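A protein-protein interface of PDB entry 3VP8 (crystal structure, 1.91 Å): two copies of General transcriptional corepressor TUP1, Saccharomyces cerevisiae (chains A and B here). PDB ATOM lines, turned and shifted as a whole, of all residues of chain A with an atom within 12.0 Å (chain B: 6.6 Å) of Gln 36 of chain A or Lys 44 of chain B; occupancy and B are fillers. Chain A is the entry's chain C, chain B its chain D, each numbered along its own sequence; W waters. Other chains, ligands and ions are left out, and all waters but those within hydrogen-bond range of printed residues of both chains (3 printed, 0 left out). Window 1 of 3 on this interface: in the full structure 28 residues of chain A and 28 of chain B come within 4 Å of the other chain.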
ATOM      1  N   GLN A  25     -23.781   6.500  -7.952  1.00  0.00           N
ATOM      2  CA  GLN A  25     -22.394   6.813  -7.569  1.00  0.00           C
ATOM      3  C   GLN A  25     -21.693   7.742  -8.567  1.00  0.00           C
ATOM      4  O   GLN A  25     -20.952   8.627  -8.163  1.00  0.00           O
ATOM      5  CB  GLN A  25     -21.558   5.538  -7.387  1.00  0.00           C
ATOM      6  CG  GLN A  25     -20.081   5.825  -7.054  1.00  0.00           C
ATOM      7  CD  GLN A  25     -19.191   4.583  -7.043  1.00  0.00           C
ATOM      8  OE1 GLN A  25     -18.330   4.432  -6.173  1.00  0.00           O
ATOM      9  NE2 GLN A  25     -19.376   3.708  -8.027  1.00  0.00           N
ATOM     10  N   VAL A  26     -21.907   7.537  -9.868  1.00  0.00           N
ATOM     11  CA  VAL A  26     -21.328   8.433 -10.878  1.00  0.00           C
ATOM     12  C   VAL A  26     -21.846   9.859 -10.678  1.00  0.00           C
ATOM     13  O   VAL A  26     -21.086  10.820 -10.727  1.00  0.00           O
ATOM     14  CB  VAL A  26     -21.635   7.955 -12.327  1.00  0.00           C
ATOM     15  CG1 VAL A  26     -21.226   9.008 -13.354  1.00  0.00           C
ATOM     16  CG2 VAL A  26     -20.910   6.651 -12.623  1.00  0.00           C
ATOM     17  N   SER A  27     -23.147   9.998 -10.451  1.00  0.00           N
ATOM     18  CA  SER A  27     -23.738  11.313 -10.241  1.00  0.00           C
ATOM     19  C   SER A  27     -23.222  11.983  -8.965  1.00  0.00           C
ATOM     20  O   SER A  27     -22.843  13.153  -8.980  1.00  0.00           O
ATOM     21  CB  SER A  27     -25.264  11.216 -10.199  1.00  0.00           C
ATOM     22  OG  SER A  27     -25.758  10.682 -11.413  1.00  0.00           O
ATOM     23  N   GLN A  28     -23.201  11.247  -7.861  1.00  0.00           N
ATOM     24  CA  GLN A  28     -22.763  11.850  -6.602  1.00  0.00           C
ATOM     25  C   GLN A  28     -21.283  12.223  -6.658  1.00  0.00           C
ATOM     26  O   GLN A  28     -20.842  13.226  -6.070  1.00  0.00           O
ATOM     27  CB  GLN A  28     -23.059  10.903  -5.433  1.00  0.00           C
ATOM     28  CG  GLN A  28     -24.559  10.577  -5.270  1.00  0.00           C
ATOM     29  CD  GLN A  28     -24.935  10.104  -3.863  1.00  0.00           C
ATOM     30  OE1 GLN A  28     -24.511   9.043  -3.410  1.00  0.00           O
ATOM     31  NE2 GLN A  28     -25.733  10.906  -3.167  1.00  0.00           N
ATOM     32  N   GLU A  29     -20.502  11.424  -7.370  1.00  0.00           N
ATOM     33  CA  GLU A  29     -19.081  11.759  -7.546  1.00  0.00           C
ATOM     34  C   GLU A  29     -18.861  12.985  -8.433  1.00  0.00           C
ATOM     35  O   GLU A  29     -17.934  13.749  -8.204  1.00  0.00           O
ATOM     36  CB  GLU A  29     -18.296  10.570  -8.093  1.00  0.00           C
ATOM     37  CG  GLU A  29     -17.849   9.602  -7.014  1.00  0.00           C
ATOM     38  CD  GLU A  29     -17.193   8.352  -7.576  1.00  0.00           C
ATOM     39  OE1 GLU A  29     -17.053   8.258  -8.813  1.00  0.00           O
ATOM     40  OE2 GLU A  29     -16.813   7.465  -6.781  1.00  0.00           O
ATOM     41  N   ALA A  30     -19.714  13.188  -9.433  1.00  0.00           N
ATOM     42  CA  ALA A  30     -19.550  14.337 -10.321  1.00  0.00           C
ATOM     43  C   ALA A  30     -19.841  15.621  -9.562  1.00  0.00           C
ATOM     44  O   ALA A  30     -19.208  16.672  -9.786  1.00  0.00           O
ATOM     45  CB  ALA A  30     -20.490  14.209 -11.521  1.00  0.00           C
ATOM     46  N   ASN A  31     -20.828  15.541  -8.675  1.00  0.00           N
ATOM     47  CA  ASN A  31     -21.207  16.690  -7.855  1.00  0.00           C
ATOM     48  C   ASN A  31     -20.101  17.057  -6.860  1.00  0.00           C
ATOM     49  O   ASN A  31     -19.793  18.228  -6.661  1.00  0.00           O
ATOM     50  CB  ASN A  31     -22.520  16.404  -7.131  1.00  0.00           C
ATOM     51  CG  ASN A  31     -23.695  16.310  -8.081  1.00  0.00           C
ATOM     52  OD1 ASN A  31     -23.668  16.886  -9.178  1.00  0.00           O
ATOM     53  ND2 ASN A  31     -24.746  15.592  -7.667  1.00  0.00           N
ATOM     54  N   THR A  32     -19.517  16.036  -6.243  1.00  0.00           N
ATOM     55  CA  THR A  32     -18.411  16.213  -5.324  1.00  0.00           C
ATOM     56  C   THR A  32     -17.221  16.833  -6.057  1.00  0.00           C
ATOM     57  O   THR A  32     -16.600  17.786  -5.569  1.00  0.00           O
ATOM     58  CB  THR A  32     -18.019  14.868  -4.705  1.00  0.00           C
ATOM     59  OG1 THR A  32     -19.114  14.376  -3.918  1.00  0.00           O
ATOM     60  CG2 THR A  32     -16.779  14.997  -3.837  1.00  0.00           C
ATOM     61  N   TYR A  33     -16.916  16.308  -7.240  1.00  0.00           N
ATOM     62  CA  TYR A  33     -15.788  16.800  -8.035  1.00  0.00           C
ATOM     63  C   TYR A  33     -15.957  18.267  -8.431  1.00  0.00           C
ATOM     64  O   TYR A  33     -14.989  19.005  -8.549  1.00  0.00           O
ATOM     65  CB  TYR A  33     -15.652  15.996  -9.327  1.00  0.00           C
ATOM     66  CG  TYR A  33     -15.047  14.617  -9.206  1.00  0.00           C
ATOM     67  CD1 TYR A  33     -15.359  13.627 -10.128  1.00  0.00           C
ATOM     68  CD2 TYR A  33     -14.143  14.308  -8.202  1.00  0.00           C
ATOM     69  CE1 TYR A  33     -14.811  12.355 -10.042  1.00  0.00           C
ATOM     70  CE2 TYR A  33     -13.581  13.033  -8.113  1.00  0.00           C
ATOM     71  CZ  TYR A  33     -13.920  12.070  -9.034  1.00  0.00           C
ATOM     72  OH  TYR A  33     -13.368  10.812  -8.957  1.00  0.00           O
ATOM     73  N   ARG A  34     -17.193  18.672  -8.693  1.00  0.00           N
ATOM     74  CA  ARG A  34     -17.456  20.004  -9.207  1.00  0.00           C
ATOM     75  C   ARG A  34     -17.085  21.033  -8.155  1.00  0.00           C
ATOM     76  O   ARG A  34     -16.459  22.055  -8.459  1.00  0.00           O
ATOM     77  CB  ARG A  34     -18.934  20.145  -9.587  1.00  0.00           C
ATOM     78  CG  ARG A  34     -19.220  21.351 -10.497  1.00  0.00           C
ATOM     79  CD  ARG A  34     -19.366  22.635  -9.722  1.00  0.00           C
ATOM     80  NE  ARG A  34     -19.940  23.714 -10.535  1.00  0.00           N
ATOM     81  CZ  ARG A  34     -20.330  24.887 -10.040  1.00  0.00           C
ATOM     82  NH1 ARG A  34     -20.214  25.118  -8.738  1.00  0.00           N
ATOM     83  NH2 ARG A  34     -20.833  25.829 -10.839  1.00  0.00           N
ATOM     84  N   LEU A  35     -17.483  20.757  -6.919  1.00  0.00           N
ATOM     85  CA  LEU A  35     -17.213  21.658  -5.806  1.00  0.00           C
ATOM     86  C   LEU A  35     -15.726  21.639  -5.444  1.00  0.00           C
ATOM     87  O   LEU A  35     -15.116  22.688  -5.174  1.00  0.00           O
ATOM     88  CB  LEU A  35     -18.052  21.252  -4.604  1.00  0.00           C
ATOM     89  CG  LEU A  35     -18.029  22.269  -3.462  1.00  0.00           C
ATOM     90  CD1 LEU A  35     -18.627  23.588  -3.936  1.00  0.00           C
ATOM     91  CD2 LEU A  35     -18.784  21.742  -2.250  1.00  0.00           C
ATOM     92  N   GLN A  36     -15.145  20.446  -5.437  1.00  0.00           N
ATOM     93  CA  GLN A  36     -13.716  20.304  -5.189  1.00  0.00           C
ATOM     94  C   GLN A  36     -12.903  21.090  -6.215  1.00  0.00           C
ATOM     95  O   GLN A  36     -11.974  21.815  -5.852  1.00  0.00           O
ATOM     96  CB  GLN A  36     -13.304  18.835  -5.241  1.00  0.00           C
ATOM     97  CG  GLN A  36     -13.720  18.013  -4.031  1.00  0.00           C
ATOM     98  CD  GLN A  36     -13.320  16.553  -4.183  1.00  0.00           C
ATOM     99  OE1 GLN A  36     -13.404  15.763  -3.234  1.00  0.00           O
ATOM    100  NE2 GLN A  36     -12.872  16.190  -5.383  1.00  0.00           N
ATOM    101  N   ASN A  37     -13.239  20.930  -7.491  1.00  0.00           N
ATOM    102  CA  ASN A  37     -12.556  21.665  -8.560  1.00  0.00           C
ATOM    103  C   ASN A  37     -12.606  23.171  -8.355  1.00  0.00           C
ATOM    104  O   ASN A  37     -11.606  23.884  -8.508  1.00  0.00           O
ATOM    105  CB  ASN A  37     -13.173  21.336  -9.924  1.00  0.00           C
ATOM    106  CG  ASN A  37     -12.412  21.978 -11.067  1.00  0.00           C
ATOM    107  OD1 ASN A  37     -11.435  21.413 -11.572  1.00  0.00           O
ATOM    108  ND2 ASN A  37     -12.845  23.170 -11.475  1.00  0.00           N
ATOM    109  N   GLN A  38     -13.789  23.662  -8.021  1.00  0.00           N
ATOM    110  CA  GLN A  38     -13.979  25.093  -7.771  1.00  0.00           C
ATOM    111  C   GLN A  38     -13.211  25.601  -6.554  1.00  0.00           C
ATOM    112  O   GLN A  38     -12.684  26.722  -6.568  1.00  0.00           O
ATOM    113  CB  GLN A  38     -15.469  25.416  -7.620  1.00  0.00           C
ATOM    114  CG  GLN A  38     -15.767  26.910  -7.807  1.00  0.00           C
ATOM    115  CD  GLN A  38     -15.409  27.408  -9.209  1.00  0.00           C
ATOM    116  OE1 GLN A  38     -15.982  26.955 -10.203  1.00  0.00           O
ATOM    117  NE2 GLN A  38     -14.453  28.339  -9.291  1.00  0.00           N
ATOM    118  N   LYS A  39     -13.158  24.802  -5.491  1.00  0.00           N
ATOM    119  CA  LYS A  39     -12.402  25.199  -4.303  1.00  0.00           C
ATOM    120  C   LYS A  39     -10.911  25.272  -4.617  1.00  0.00           C
ATOM    121  O   LYS A  39     -10.216  26.195  -4.195  1.00  0.00           O
ATOM    122  CB  LYS A  39     -12.658  24.238  -3.139  1.00  0.00           C
ATOM    123  CG  LYS A  39     -14.087  24.309  -2.571  1.00  0.00           C
ATOM    124  CD  LYS A  39     -14.267  23.336  -1.414  1.00  0.00           C
ATOM    125  CE  LYS A  39     -15.706  23.355  -0.886  1.00  0.00           C
ATOM    126  NZ  LYS A  39     -15.930  22.310   0.166  1.00  0.00           N
ATOM    127  N   ASP A  40     -10.428  24.302  -5.384  1.00  0.00           N
ATOM    128  CA  ASP A  40      -9.031  24.292  -5.815  1.00  0.00           C
ATOM    129  C   ASP A  40      -8.705  25.493  -6.695  1.00  0.00           C
ATOM    130  O   ASP A  40      -7.708  26.198  -6.472  1.00  0.00           O
ATOM    131  CB  ASP A  40      -8.722  22.987  -6.570  1.00  0.00           C
ATOM    132  CG  ASP A  40      -7.229  22.767  -6.746  1.00  0.00           C
ATOM    133  OD1 ASP A  40      -6.668  23.267  -7.740  1.00  0.00           O
ATOM    134  OD2 ASP A  40      -6.617  22.108  -5.880  1.00  0.00           O
ATOM    135  N   TYR A  41      -9.551  25.737  -7.685  1.00  0.00           N
ATOM    136  CA  TYR A  41      -9.400  26.892  -8.565  1.00  0.00           C
ATOM    137  C   TYR A  41      -9.407  28.186  -7.761  1.00  0.00           C
ATOM    138  O   TYR A  41      -8.550  29.065  -7.937  1.00  0.00           O
ATOM    139  CB  TYR A  41     -10.548  26.946  -9.583  1.00  0.00           C
ATOM    140  CG  TYR A  41     -10.356  28.071 -10.580  1.00  0.00           C
ATOM    141  CD1 TYR A  41     -10.613  29.392 -10.234  1.00  0.00           C
ATOM    142  CD2 TYR A  41      -9.894  27.812 -11.860  1.00  0.00           C
ATOM    143  CE1 TYR A  41     -10.425  30.421 -11.143  1.00  0.00           C
ATOM    144  CE2 TYR A  41      -9.693  28.829 -12.772  1.00  0.00           C
ATOM    145  CZ  TYR A  41      -9.958  30.133 -12.416  1.00  0.00           C
ATOM    146  OH  TYR A  41      -9.749  31.149 -13.344  1.00  0.00           O
ATOM    147  N   ASP A  42     -10.384  28.309  -6.876  1.00  0.00           N
ATOM    148  CA  ASP A  42     -10.544  29.544  -6.102  1.00  0.00           C
ATOM    149  C   ASP A  42      -9.403  29.809  -5.124  1.00  0.00           C
ATOM    150  O   ASP A  42      -9.028  30.962  -4.909  1.00  0.00           O
ATOM    151  CB  ASP A  42     -11.884  29.543  -5.360  1.00  0.00           C
ATOM    152  CG  ASP A  42     -13.072  29.687  -6.309  1.00  0.00           C
ATOM    153  OD1 ASP A  42     -12.856  30.116  -7.465  1.00  0.00           O
ATOM    154  OD2 ASP A  42     -14.219  29.381  -5.891  1.00  0.00           O
ATOM    155  N   PHE A  43      -8.859  28.754  -4.528  1.00  0.00           N
ATOM    156  CA  PHE A  43      -7.709  28.917  -3.646  1.00  0.00           C
ATOM    157  C   PHE A  43      -6.501  29.435  -4.417  1.00  0.00           C
ATOM    158  O   PHE A  43      -5.780  30.302  -3.936  1.00  0.00           O
ATOM    159  CB  PHE A  43      -7.306  27.614  -2.936  1.00  0.00           C
ATOM    160  CG  PHE A  43      -5.927  27.688  -2.345  1.00  0.00           C
ATOM    161  CD1 PHE A  43      -4.836  27.149  -3.009  1.00  0.00           C
ATOM    162  CD2 PHE A  43      -5.707  28.409  -1.181  1.00  0.00           C
ATOM    163  CE1 PHE A  43      -3.546  27.284  -2.479  1.00  0.00           C
ATOM    164  CE2 PHE A  43      -4.437  28.535  -0.640  1.00  0.00           C
ATOM    165  CZ  PHE A  43      -3.352  27.969  -1.289  1.00  0.00           C
ATOM    166  N   LYS A  44      -6.264  28.891  -5.607  1.00  0.00           N
ATOM    167  CA  LYS A  44      -5.108  29.317  -6.411  1.00  0.00           C
ATOM    168  C   LYS A  44      -5.287  30.706  -7.013  1.00  0.00           C
ATOM    169  O   LYS A  44      -4.326  31.485  -7.162  1.00  0.00           O
ATOM    170  CB  LYS A  44      -4.797  28.255  -7.469  1.00  0.00           C
ATOM    171  CG  LYS A  44      -4.406  26.943  -6.832  1.00  0.00           C
ATOM    172  CD  LYS A  44      -4.272  25.816  -7.862  1.00  0.00           C
ATOM    173  CE  LYS A  44      -3.663  24.601  -7.200  1.00  0.00           C
ATOM    174  NZ  LYS A  44      -4.016  23.327  -7.922  1.00  0.00           N
ATOM    175  N   MET A  45      -6.534  31.040  -7.317  1.00  0.00           N
ATOM    176  CA  MET A  45      -6.858  32.386  -7.795  1.00  0.00           C
ATOM    177  C   MET A  45      -6.650  33.405  -6.699  1.00  0.00           C
ATOM    178  O   MET A  45      -6.044  34.450  -6.927  1.00  0.00           O
ATOM    179  CB  MET A  45      -8.322  32.479  -8.260  1.00  0.00           C
ATOM    180  CG  MET A  45      -8.798  33.919  -8.528  1.00  0.00           C
ATOM    181  SD  MET A  45     -10.569  33.994  -8.933  1.00  0.00           S
ATOM    182  CE  MET A  45     -11.300  33.918  -7.294  1.00  0.00           C
ATOM    183  N   ASN A  46      -7.157  33.108  -5.507  1.00  0.00           N
ATOM    184  CA  ASN A  46      -7.043  34.038  -4.382  1.00  0.00           C
ATOM    185  C   ASN A  46      -5.613  34.162  -3.862  1.00  0.00           C
ATOM    186  O   ASN A  46      -5.171  35.235  -3.427  1.00  0.00           O
ATOM    187  CB  ASN A  46      -8.028  33.656  -3.266  1.00  0.00           C
ATOM    188  CG  ASN A  46      -9.466  34.031  -3.613  1.00  0.00           C
ATOM    189  OD1 ASN A  46      -9.699  35.040  -4.274  1.00  0.00           O
ATOM    190  ND2 ASN A  46     -10.430  33.217  -3.182  1.00  0.00           N
ATOM    191  N   LYS B  39      -2.148  16.097 -13.003  1.00  0.00           N
ATOM    192  CA  LYS B  39      -2.279  14.980 -12.082  1.00  0.00           C
ATOM    193  C   LYS B  39      -3.695  14.847 -11.544  1.00  0.00           C
ATOM    194  O   LYS B  39      -4.245  13.738 -11.475  1.00  0.00           O
ATOM    195  CB  LYS B  39      -1.290  15.126 -10.921  1.00  0.00           C
ATOM    196  CG  LYS B  39      -1.428  14.031  -9.883  1.00  0.00           C
ATOM    197  CD  LYS B  39      -0.443  14.201  -8.717  1.00  0.00           C
ATOM    198  CE  LYS B  39      -0.781  13.227  -7.569  1.00  0.00           C
ATOM    199  NZ  LYS B  39       0.189  13.325  -6.442  1.00  0.00           N
ATOM    200  N   ASP B  40      -4.281  15.972 -11.145  1.00  0.00           N
ATOM    201  CA  ASP B  40      -5.640  15.969 -10.606  1.00  0.00           C
ATOM    202  C   ASP B  40      -6.650  15.586 -11.684  1.00  0.00           C
ATOM    203  O   ASP B  40      -7.559  14.799 -11.443  1.00  0.00           O
ATOM    204  CB  ASP B  40      -6.011  17.350 -10.087  1.00  0.00           C
ATOM    205  CG  ASP B  40      -5.231  17.748  -8.849  1.00  0.00           C
ATOM    206  OD1 ASP B  40      -4.547  16.891  -8.247  1.00  0.00           O
ATOM    207  OD2 ASP B  40      -5.327  18.934  -8.484  1.00  0.00           O
ATOM    208  N   TYR B  41      -6.491  16.157 -12.872  1.00  0.00           N
ATOM    209  CA  TYR B  41      -7.398  15.840 -13.976  1.00  0.00           C
ATOM    210  C   TYR B  41      -7.386  14.339 -14.312  1.00  0.00           C
ATOM    211  O   TYR B  41      -8.442  13.675 -14.469  1.00  0.00           O
ATOM    212  CB  TYR B  41      -7.015  16.646 -15.226  1.00  0.00           C
ATOM    213  CG  TYR B  41      -8.059  16.504 -16.318  1.00  0.00           C
ATOM    214  CD1 TYR B  41      -8.087  15.391 -17.144  1.00  0.00           C
ATOM    215  CD2 TYR B  41      -9.047  17.461 -16.483  1.00  0.00           C
ATOM    216  CE1 TYR B  41      -9.074  15.252 -18.149  1.00  0.00           C
ATOM    217  CE2 TYR B  41     -10.036  17.343 -17.476  1.00  0.00           C
ATOM    218  CZ  TYR B  41     -10.044  16.237 -18.309  1.00  0.00           C
ATOM    219  OH  TYR B  41     -11.045  16.122 -19.282  1.00  0.00           O
ATOM    220  N   ASP B  42      -6.182  13.796 -14.416  1.00  0.00           N
ATOM    221  CA  ASP B  42      -6.023  12.379 -14.741  1.00  0.00           C
ATOM    222  C   ASP B  42      -6.615  11.448 -13.684  1.00  0.00           C
ATOM    223  O   ASP B  42      -7.241  10.455 -14.024  1.00  0.00           O
ATOM    224  CB  ASP B  42      -4.554  12.031 -15.002  1.00  0.00           C
ATOM    225  CG  ASP B  42      -4.057  12.586 -16.317  1.00  0.00           C
ATOM    226  OD1 ASP B  42      -4.886  12.985 -17.167  1.00  0.00           O
ATOM    227  OD2 ASP B  42      -2.836  12.628 -16.511  1.00  0.00           O
ATOM    228  N   PHE B  43      -6.426  11.764 -12.407  1.00  0.00           N
ATOM    229  CA  PHE B  43      -7.026  10.941 -11.362  1.00  0.00           C
ATOM    230  C   PHE B  43      -8.557  10.824 -11.517  1.00  0.00           C
ATOM    231  O   PHE B  43      -9.123   9.729 -11.479  1.00  0.00           O
ATOM    232  CB  PHE B  43      -6.690  11.487  -9.974  1.00  0.00           C
ATOM    233  CG  PHE B  43      -7.406  10.765  -8.870  1.00  0.00           C
ATOM    234  CD1 PHE B  43      -6.990   9.504  -8.466  1.00  0.00           C
ATOM    235  CD2 PHE B  43      -8.522  11.328  -8.268  1.00  0.00           C
ATOM    236  CE1 PHE B  43      -7.665   8.820  -7.457  1.00  0.00           C
ATOM    237  CE2 PHE B  43      -9.205  10.654  -7.263  1.00  0.00           C
ATOM    238  CZ  PHE B  43      -8.774   9.399  -6.854  1.00  0.00           C
ATOM    239  N   LYS B  44      -9.223  11.960 -11.684  1.00  0.00           N
ATOM    240  CA  LYS B  44     -10.672  11.978 -11.844  1.00  0.00           C
ATOM    241  C   LYS B  44     -11.106  11.326 -13.153  1.00  0.00           C
ATOM    242  O   LYS B  44     -12.072  10.572 -13.193  1.00  0.00           O
ATOM    243  CB  LYS B  44     -11.189  13.413 -11.802  1.00  0.00           C
ATOM    244  CG  LYS B  44     -10.863  14.165 -10.518  1.00  0.00           C
ATOM    245  CD  LYS B  44     -11.547  15.536 -10.491  1.00  0.00           C
ATOM    246  CE  LYS B  44     -11.322  16.230  -9.154  1.00  0.00           C
ATOM    247  NZ  LYS B  44     -12.337  17.299  -8.920  1.00  0.00           N
ATOM    248  N   MET B  45     -10.403  11.654 -14.230  1.00  0.00           N
ATOM    249  CA  MET B  45     -10.701  11.099 -15.541  1.00  0.00           C
ATOM    250  C   MET B  45     -10.693   9.581 -15.478  1.00  0.00           C
ATOM    251  O   MET B  45     -11.620   8.930 -15.947  1.00  0.00           O
ATOM    252  CB  MET B  45      -9.672  11.566 -16.575  1.00  0.00           C
ATOM    253  CG  MET B  45      -9.961  11.059 -18.003  1.00  0.00           C
ATOM    254  SD  MET B  45      -8.615  11.471 -19.126  1.00  0.00           S
ATOM    255  CE  MET B  45      -7.272  10.438 -18.521  1.00  0.00           C
ATOM    256  N   ASN B  46      -9.639   9.028 -14.888  1.00  0.00           N
ATOM    257  CA  ASN B  46      -9.463   7.586 -14.812  1.00  0.00           C
ATOM    258  C   ASN B  46     -10.528   6.954 -13.930  1.00  0.00           C
ATOM    259  O   ASN B  46     -10.989   5.847 -14.202  1.00  0.00           O
ATOM    260  CB  ASN B  46      -8.074   7.248 -14.276  1.00  0.00           C
ATOM    261  CG  ASN B  46      -7.012   7.303 -15.350  1.00  0.00           C
ATOM    262  OD1 ASN B  46      -7.018   6.496 -16.280  1.00  0.00           O
ATOM    263  ND2 ASN B  46      -6.083   8.240 -15.223  1.00  0.00           N
ATOM    264  N   GLN B  47     -10.922   7.656 -12.872  1.00  0.00           N
ATOM    265  CA  GLN B  47     -11.968   7.129 -12.015  1.00  0.00           C
ATOM    266  C   GLN B  47     -13.291   7.034 -12.777  1.00  0.00           C
ATOM    267  O   GLN B  47     -14.035   6.043 -12.659  1.00  0.00           O
ATOM    268  CB  GLN B  47     -12.136   7.992 -10.776  1.00  0.00           C
ATOM    269  CG  GLN B  47     -13.252   7.525  -9.860  1.00  0.00           C
ATOM    270  CD  GLN B  47     -13.119   8.079  -8.450  1.00  0.00           C
ATOM    271  OE1 GLN B  47     -14.112   8.460  -7.827  1.00  0.00           O
ATOM    272  NE2 GLN B  47     -11.889   8.113  -7.934  1.00  0.00           N
ATOM    273  N   GLN B  48     -13.587   8.070 -13.554  1.00  0.00           N
ATOM    274  CA  GLN B  48     -14.849   8.131 -14.278  1.00  0.00           C
ATOM    275  C   GLN B  48     -14.866   7.102 -15.406  1.00  0.00           C
ATOM    276  O   GLN B  48     -15.922   6.607 -15.781  1.00  0.00           O
ATOM    277  CB  GLN B  48     -15.097   9.552 -14.802  1.00  0.00           C
ATOM    278  CG  GLN B  48     -15.465  10.523 -13.688  1.00  0.00           C
ATOM    279  CD  GLN B  48     -15.572  11.968 -14.156  1.00  0.00           C
ATOM    280  OE1 GLN B  48     -14.804  12.420 -15.009  1.00  0.00           O
ATOM    281  NE2 GLN B  48     -16.525  12.706 -13.587  1.00  0.00           N
ATOM    282  N   LEU B  49     -13.686   6.798 -15.943  1.00  0.00           N
ATOM    283  CA  LEU B  49     -13.526   5.786 -16.996  1.00  0.00           C
ATOM    284  C   LEU B  49     -13.775   4.385 -16.452  1.00  0.00           C
ATOM    285  O   LEU B  49     -14.413   3.568 -17.097  1.00  0.00           O
ATOM    286  CB  LEU B  49     -12.103   5.841 -17.555  1.00  0.00           C
ATOM    287  CG  LEU B  49     -11.819   6.986 -18.519  1.00  0.00           C
ATOM    288  CD1 LEU B  49     -10.303   7.243 -18.617  1.00  0.00           C
ATOM    289  CD2 LEU B  49     -12.407   6.672 -19.885  1.00  0.00           C
HETATM  290  O   HOH W   1      -4.266  20.660  -6.799  1.00  0.00           O
HETATM  291  O   HOH W   2     -13.110  18.268 -11.180  1.00  0.00           O
HETATM  292  O   HOH W   3     -18.765  10.958 -12.226  1.00  0.00           O
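8 positions are printed for both chains.
NZ of Lys 44 of chain B lies within hydrogen-bond range of O of Tyr 33 of chain A (3.2 Å).
OH of Tyr 33 of chain A lies within hydrogen-bond range of OE1 of Gln 47 of chain B (2.7 Å).
OE2 of Glu 29 of chain A sits close to OE1 of Gln 47 of chain B, 3.1 Å away.
OE2 of Glu 29 of chain A lies close to OE1 of Gln 25 of chain A, at 3.4 Å.
Tyr 33 of chain A touches Gln 48 of chain B (CD1 to NE2, 3.8 Å).
Gln 36 of chain A touches Lys 44 of chain B (NE2 to NZ, 3.7 Å).
Water W2 lies within hydrogen-bond range of NZ of Lys 44 of chain B and O of Tyr 33 of chain A.
Water W1 lies within hydrogen-bond range of OD2 of Asp 40 of chain B (2.6 Å), NZ of Lys 44 of chain A (2.9 Å) and OD2 of Asp 40 of chain A (2.9 Å).
Water W3 bridges the backbone carbonyl oxygen of Val 26 of chain A (2.8 Å) and the side-chain amide nitrogen of Gln 48 of chain B (3.2 Å).
Printed residues of chain B that touch a printed residue of chain A: Lys 44, Gln 47 and Gln 48.
Of the 22 printed residues of chain A, 3 touch a printed residue of chain B.
Hydrophobic or aromatic side chains of chain A that line the printed part of chain B: Tyr 33.
Among the printed residues, 5 pairs touch across the chains.
Among the printed residues, no Asp or Glu carboxylate lies within 4 Å of a Lys or Arg side-chain nitrogen of the other chain.
Of the printed residues of chain B, Glu 29 of chain A touches Gln 47 (3.1 Å).
Of the printed residues of chain B, Tyr 33 of chain A touches Lys 44 (3.2 Å), Gln 47 (2.7 Å) and Gln 48 (3.8 Å).
Asp 40 of chain B touches none of the printed residues of chain A.
No residue of chain A comes within 4 Å of Phe 43 of chain B.
Printed residues of chain A within 4 Å of Lys 44 of chain B: Tyr 33 and Gln 36.
No residue of chain A comes within 4 Å of Asn 46 of chain B.
The nearest printed residue of chain B that does not touch Glu 29 of chain A is Gln 48 of chain B (5.6 Å).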
